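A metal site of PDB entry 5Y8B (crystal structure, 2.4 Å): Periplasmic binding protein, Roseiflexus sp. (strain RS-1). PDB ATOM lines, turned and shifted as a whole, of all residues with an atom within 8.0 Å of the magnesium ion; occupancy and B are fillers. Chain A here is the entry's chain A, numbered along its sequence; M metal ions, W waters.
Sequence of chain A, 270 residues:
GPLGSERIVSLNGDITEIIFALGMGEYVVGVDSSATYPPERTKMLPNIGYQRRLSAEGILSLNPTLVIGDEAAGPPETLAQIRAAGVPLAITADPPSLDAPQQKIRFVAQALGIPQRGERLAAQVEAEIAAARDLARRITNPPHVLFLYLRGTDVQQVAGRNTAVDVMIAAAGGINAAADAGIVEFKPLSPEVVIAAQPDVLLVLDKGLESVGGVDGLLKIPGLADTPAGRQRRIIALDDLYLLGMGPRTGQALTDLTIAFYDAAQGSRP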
ATOM      1  N   ASN A  12      21.566 -28.331   0.973  1.00  0.00           N
ATOM      2  CA  ASN A  12      22.559 -29.241   1.569  1.00  0.00           C
ATOM      3  C   ASN A  12      21.920 -30.006   2.736  1.00  0.00           C
ATOM      4  O   ASN A  12      21.090 -29.451   3.460  1.00  0.00           O
ATOM      5  CB  ASN A  12      23.826 -28.485   2.025  1.00  0.00           C
ATOM      6  CG  ASN A  12      24.305 -27.460   0.986  1.00  0.00           C
ATOM      7  OD1 ASN A  12      23.827 -26.310   0.965  1.00  0.00           O
ATOM      8  ND2 ASN A  12      25.231 -27.871   0.105  1.00  0.00           N
ATOM      9  N   GLY A  13      22.315 -31.265   2.879  1.00  0.00           N
ATOM     10  CA  GLY A  13      21.749 -32.162   3.879  1.00  0.00           C
ATOM     11  C   GLY A  13      21.870 -31.689   5.325  1.00  0.00           C
ATOM     12  O   GLY A  13      20.939 -31.869   6.106  1.00  0.00           O
ATOM     13  N   ASP A  14      23.021 -31.105   5.664  1.00  0.00           N
ATOM     14  CA  ASP A  14      23.232 -30.585   7.018  1.00  0.00           C
ATOM     15  C   ASP A  14      22.326 -29.398   7.329  1.00  0.00           C
ATOM     16  O   ASP A  14      21.749 -29.334   8.426  1.00  0.00           O
ATOM     17  CB  ASP A  14      24.715 -30.259   7.272  1.00  0.00           C
ATOM     18  CG  ASP A  14      25.300 -29.272   6.266  1.00  0.00           C
ATOM     19  OD1 ASP A  14      24.891 -29.255   5.099  1.00  0.00           O
ATOM     20  OD2 ASP A  14      26.218 -28.510   6.642  1.00  0.00           O
ATOM     21  N   ILE A  15      22.166 -28.510   6.346  1.00  0.00           N
ATOM     22  CA  ILE A  15      21.211 -27.391   6.401  1.00  0.00           C
ATOM     23  C   ILE A  15      19.768 -27.913   6.611  1.00  0.00           C
ATOM     24  O   ILE A  15      19.036 -27.399   7.450  1.00  0.00           O
ATOM     25  CB  ILE A  15      21.340 -26.467   5.154  1.00  0.00           C
ATOM     26  CG1 ILE A  15      22.744 -25.821   5.037  1.00  0.00           C
ATOM     27  CG2 ILE A  15      20.228 -25.419   5.093  1.00  0.00           C
ATOM     28  CD1 ILE A  15      23.223 -24.971   6.204  1.00  0.00           C
ATOM     29  N   ILE A  18      19.377 -29.200  10.172  1.00  0.00           N
ATOM     30  CA  ILE A  18      19.197 -28.028  11.052  1.00  0.00           C
ATOM     31  C   ILE A  18      17.753 -27.511  11.032  1.00  0.00           C
ATOM     32  O   ILE A  18      17.202 -27.190  12.102  1.00  0.00           O
ATOM     33  CB  ILE A  18      20.208 -26.890  10.727  1.00  0.00           C
ATOM     34  CG1 ILE A  18      21.637 -27.350  11.019  1.00  0.00           C
ATOM     35  CG2 ILE A  18      19.946 -25.635  11.559  1.00  0.00           C
ATOM     36  CD1 ILE A  18      22.707 -26.526  10.351  1.00  0.00           C
ATOM     37  N   SER A  34      21.773 -35.488  -0.510  1.00  0.00           N
ATOM     38  CA  SER A  34      22.525 -35.752   0.701  1.00  0.00           C
ATOM     39  C   SER A  34      21.687 -35.585   1.961  1.00  0.00           C
ATOM     40  O   SER A  34      22.182 -35.822   3.064  1.00  0.00           O
ATOM     41  CB  SER A  34      23.767 -34.856   0.756  1.00  0.00           C
ATOM     42  OG  SER A  34      23.419 -33.515   1.083  1.00  0.00           O
ATOM     43  N   GLN A  51      23.969 -31.630  -4.671  1.00  0.00           N
ATOM     44  CA  GLN A  51      24.238 -30.306  -4.091  1.00  0.00           C
ATOM     45  C   GLN A  51      25.257 -29.458  -4.855  1.00  0.00           C
ATOM     46  O   GLN A  51      25.153 -28.242  -4.864  1.00  0.00           O
ATOM     47  CB  GLN A  51      24.606 -30.402  -2.582  1.00  0.00           C
ATOM     48  CG  GLN A  51      25.969 -31.015  -2.294  1.00  0.00           C
ATOM     49  CD  GLN A  51      26.139 -31.481  -0.860  1.00  0.00           C
ATOM     50  OE1 GLN A  51      26.059 -30.692   0.081  1.00  0.00           O
ATOM     51  NE2 GLN A  51      26.434 -32.766  -0.685  1.00  0.00           N
ATOM     52  N   ARG A  52      26.218 -30.120  -5.523  1.00  0.00           N
ATOM     53  CA  ARG A  52      27.268 -29.451  -6.296  1.00  0.00           C
ATOM     54  C   ARG A  52      26.930 -29.282  -7.785  1.00  0.00           C
ATOM     55  O   ARG A  52      27.658 -28.600  -8.504  1.00  0.00           O
ATOM     56  CB  ARG A  52      28.601 -30.193  -6.158  1.00  0.00           C
ATOM     57  CG  ARG A  52      29.309 -29.981  -4.830  1.00  0.00           C
ATOM     58  CD  ARG A  52      30.510 -30.909  -4.658  1.00  0.00           C
ATOM     59  NE  ARG A  52      30.817 -31.124  -3.251  1.00  0.00           N
ATOM     60  CZ  ARG A  52      30.391 -32.167  -2.518  1.00  0.00           C
ATOM     61  NH1 ARG A  52      29.649 -33.118  -3.041  1.00  0.00           N
ATOM     62  NH2 ARG A  52      30.735 -32.237  -1.240  1.00  0.00           N
ATOM     63  N   GLY A  69      21.270 -22.603   1.853  1.00  0.00           N
ATOM     64  CA  GLY A  69      22.340 -23.606   1.784  1.00  0.00           C
ATOM     65  C   GLY A  69      23.657 -23.158   2.404  1.00  0.00           C
ATOM     66  O   GLY A  69      23.733 -22.135   3.073  1.00  0.00           O
ATOM     67  N   ASP A  70      24.701 -23.953   2.201  1.00  0.00           N
ATOM     68  CA  ASP A  70      26.051 -23.538   2.576  1.00  0.00           C
ATOM     69  C   ASP A  70      27.006 -23.493   1.372  1.00  0.00           C
ATOM     70  O   ASP A  70      26.601 -23.782   0.245  1.00  0.00           O
ATOM     71  CB  ASP A  70      26.601 -24.403   3.745  1.00  0.00           C
ATOM     72  CG  ASP A  70      26.750 -25.878   3.380  1.00  0.00           C
ATOM     73  OD1 ASP A  70      26.975 -26.217   2.205  1.00  0.00           O
ATOM     74  OD2 ASP A  70      26.666 -26.716   4.306  1.00  0.00           O
ATOM     75  N   GLU A  71      28.264 -23.132   1.626  1.00  0.00           N
ATOM     76  CA  GLU A  71      29.295 -23.032   0.573  1.00  0.00           C
ATOM     77  C   GLU A  71      29.520 -24.293  -0.298  1.00  0.00           C
ATOM     78  O   GLU A  71      30.103 -24.187  -1.372  1.00  0.00           O
ATOM     79  CB  GLU A  71      30.611 -22.458   1.135  1.00  0.00           C
ATOM     80  CG  GLU A  71      31.327 -23.330   2.158  1.00  0.00           C
ATOM     81  CD  GLU A  71      32.561 -22.647   2.730  1.00  0.00           C
ATOM     82  OE1 GLU A  71      32.522 -22.242   3.906  1.00  0.00           O
ATOM     83  OE2 GLU A  71      33.578 -22.501   2.004  1.00  0.00           O
ATOM     84  N   ALA A  72      29.051 -25.466   0.134  1.00  0.00           N
ATOM     85  CA  ALA A  72      29.168 -26.673  -0.700  1.00  0.00           C
ATOM     86  C   ALA A  72      28.193 -26.701  -1.885  1.00  0.00           C
ATOM     87  O   ALA A  72      28.458 -27.377  -2.875  1.00  0.00           O
ATOM     88  CB  ALA A  72      29.051 -27.952   0.118  1.00  0.00           C
ATOM     89  N   ALA A  73      27.090 -25.960  -1.785  1.00  0.00           N
ATOM     90  CA  ALA A  73      26.092 -25.854  -2.850  1.00  0.00           C
ATOM     91  C   ALA A  73      26.639 -25.119  -4.078  1.00  0.00           C
ATOM     92  O   ALA A  73      27.273 -24.077  -3.960  1.00  0.00           O
ATOM     93  CB  ALA A  73      24.862 -25.133  -2.324  1.00  0.00           C
ATOM     94  N   THR A  92      25.421 -19.892   3.738  1.00  0.00           N
ATOM     95  CA  THR A  92      26.372 -19.792   4.868  1.00  0.00           C
ATOM     96  C   THR A  92      27.721 -20.443   4.577  1.00  0.00           C
ATOM     97  O   THR A  92      27.815 -21.327   3.725  1.00  0.00           O
ATOM     98  CB  THR A  92      25.797 -20.348   6.193  1.00  0.00           C
ATOM     99  OG1 THR A  92      26.772 -20.239   7.224  1.00  0.00           O
ATOM    100  CG2 THR A  92      25.357 -21.816   6.085  1.00  0.00           C
ATOM    101  N   ALA A  93      28.747 -19.998   5.300  1.00  0.00           N
ATOM    102  CA  ALA A  93      30.035 -20.670   5.279  1.00  0.00           C
ATOM    103  C   ALA A  93      29.923 -21.997   6.043  1.00  0.00           C
ATOM    104  O   ALA A  93      29.117 -22.124   6.963  1.00  0.00           O
ATOM    105  CB  ALA A  93      31.130 -19.798   5.880  1.00  0.00           C
ATOM    106  N   ASP A  94      30.723 -22.963   5.627  1.00  0.00           N
ATOM    107  CA  ASP A  94      30.799 -24.248   6.308  1.00  0.00           C
ATOM    108  C   ASP A  94      32.279 -24.642   6.442  1.00  0.00           C
ATOM    109  O   ASP A  94      32.772 -25.462   5.668  1.00  0.00           O
ATOM    110  CB  ASP A  94      29.968 -25.313   5.576  1.00  0.00           C
ATOM    111  CG  ASP A  94      29.666 -26.524   6.436  1.00  0.00           C
ATOM    112  OD1 ASP A  94      30.071 -26.578   7.621  1.00  0.00           O
ATOM    113  OD2 ASP A  94      28.988 -27.452   5.921  1.00  0.00           O
ATOM    114  N   PRO A  95      32.989 -24.024   7.407  1.00  0.00           N
ATOM    115  CA  PRO A  95      34.418 -24.292   7.528  1.00  0.00           C
ATOM    116  C   PRO A  95      34.708 -25.684   8.126  1.00  0.00           C
ATOM    117  O   PRO A  95      33.886 -26.193   8.893  1.00  0.00           O
ATOM    118  CB  PRO A  95      34.905 -23.199   8.472  1.00  0.00           C
ATOM    119  CG  PRO A  95      33.717 -22.836   9.291  1.00  0.00           C
ATOM    120  CD  PRO A  95      32.522 -23.037   8.406  1.00  0.00           C
ATOM    121  N   ALA A 100      31.716 -25.108  13.013  1.00  0.00           N
ATOM    122  CA  ALA A 100      30.737 -25.105  11.923  1.00  0.00           C
ATOM    123  C   ALA A 100      29.285 -25.438  12.346  1.00  0.00           C
ATOM    124  O   ALA A 100      28.373 -24.739  11.880  1.00  0.00           O
ATOM    125  CB  ALA A 100      31.182 -25.992  10.783  1.00  0.00           C
ATOM    126  N   LYS A 104      26.277 -22.643  11.631  1.00  0.00           N
ATOM    127  CA  LYS A 104      25.196 -22.948  10.688  1.00  0.00           C
ATOM    128  C   LYS A 104      23.807 -22.919  11.349  1.00  0.00           C
ATOM    129  O   LYS A 104      22.849 -22.441  10.747  1.00  0.00           O
ATOM    130  CB  LYS A 104      25.449 -24.275   9.972  1.00  0.00           C
ATOM    131  CG  LYS A 104      26.636 -24.246   9.014  1.00  0.00           C
ATOM    132  CD  LYS A 104      26.852 -25.582   8.325  1.00  0.00           C
ATOM    133  CE  LYS A 104      27.298 -26.646   9.313  1.00  0.00           C
ATOM    134  NZ  LYS A 104      27.830 -27.861   8.627  1.00  0.00           N
ATOM    135  N   LEU A 241      26.564 -37.749   5.732  1.00  0.00           N
ATOM    136  CA  LEU A 241      25.936 -36.671   6.475  1.00  0.00           C
ATOM    137  C   LEU A 241      26.274 -36.682   7.978  1.00  0.00           C
ATOM    138  O   LEU A 241      26.607 -35.643   8.550  1.00  0.00           O
ATOM    139  CB  LEU A 241      24.415 -36.726   6.270  1.00  0.00           C
ATOM    140  CG  LEU A 241      23.593 -35.605   6.898  1.00  0.00           C
ATOM    141  CD1 LEU A 241      24.083 -34.244   6.419  1.00  0.00           C
ATOM    142  CD2 LEU A 241      22.117 -35.806   6.604  1.00  0.00           C
ATOM    143  N   LEU A 244      30.541 -36.347   8.056  1.00  0.00           N
ATOM    144  CA  LEU A 244      31.157 -35.200   7.384  1.00  0.00           C
ATOM    145  C   LEU A 244      30.364 -33.878   7.415  1.00  0.00           C
ATOM    146  O   LEU A 244      30.935 -32.818   7.209  1.00  0.00           O
ATOM    147  CB  LEU A 244      31.495 -35.556   5.929  1.00  0.00           C
ATOM    148  CG  LEU A 244      32.245 -36.857   5.597  1.00  0.00           C
ATOM    149  CD1 LEU A 244      32.351 -37.073   4.095  1.00  0.00           C
ATOM    150  CD2 LEU A 244      33.619 -36.890   6.238  1.00  0.00           C
ATOM    151  N   GLY A 245      29.072 -33.972   7.699  1.00  0.00           N
ATOM    152  CA  GLY A 245      28.145 -32.847   7.585  1.00  0.00           C
ATOM    153  C   GLY A 245      28.280 -31.697   8.559  1.00  0.00           C
ATOM    154  O   GLY A 245      27.905 -30.574   8.240  1.00  0.00           O
ATOM    155  N   MET A 246      28.800 -31.974   9.756  1.00  0.00           N
ATOM    156  CA  MET A 246      28.960 -30.979  10.828  1.00  0.00           C
ATOM    157  C   MET A 246      27.611 -30.326  11.198  1.00  0.00           C
ATOM    158  O   MET A 246      27.485 -29.096  11.269  1.00  0.00           O
ATOM    159  CB  MET A 246      30.076 -29.948  10.493  1.00  0.00           C
ATOM    160  CG  MET A 246      31.486 -30.524  10.430  1.00  0.00           C
ATOM    161  SD  MET A 246      32.100 -30.957  12.073  1.00  0.00           S
ATOM    162  CE  MET A 246      33.835 -31.237  11.723  1.00  0.00           C
ATOM    163  N   GLY A 247      26.623 -31.180  11.433  1.00  0.00           N
ATOM    164  CA  GLY A 247      25.271 -30.763  11.790  1.00  0.00           C
ATOM    165  C   GLY A 247      24.963 -30.997  13.250  1.00  0.00           C
ATOM    166  O   GLY A 247      25.876 -31.255  14.030  1.00  0.00           O
HETATM  167 MG    MG M   1      27.703 -28.519   4.755  1.00  0.00          MG
HETATM  168  O   HOH W   1      28.427 -30.364   5.423  1.00  0.00           O
HETATM  169  O   HOH W   2      27.152 -29.061   2.642  1.00  0.00           O
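The side-chain carboxylate (OD2) of Asp 14 sits close to the side-chain amino group (NZ) of Lys 104 (2.6 Å). The side-chain carboxylate of Glu 71 is in hydrogen-bond range of the backbone NH of Asp 94 (2.6 Å). OD1 of Asp 94 is in salt-bridge range of NZ of Lys 104, 2.8 Å away. The side-chain amino group (NZ) of Lys 104 sits at hydrogen-bond distance from the backbone carbonyl oxygen (O) of Gly 245 (2.7 Å). The side-chain carboxylate of Asp 70 sits at hydrogen-bond distance from the backbone NH of Ala 72 (3.0 Å). The backbone carbonyl oxygen (O) of Met 246 sits at hydrogen-bond distance from the side-chain amino group (NZ) of Lys 104 (2.9 Å). N of Asp 70 sits at hydrogen-bond distance from OD1 of Asn 12 (2.8 Å).
NZ of Lys 104 touches the magnesium ion (3.9 Å). Along chain A the residues within 4 Å of the magnesium ion span positions 14 to 104. The nearest printed residue that does not touch the magnesium ion is Gly 245 (4.1 Å).
OD2 of Asp 94 binds the magnesium ion (2.0 Å). Water W1 binds the magnesium ion (2.1 Å). The magnesium ion is bound by the side-chain carboxylate (OD2) of Asp 70 (2.1 Å). Water W2 binds the magnesium ion, 2.2 Å away. OD2 of Asp 14 binds the magnesium ion (2.4 Å).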
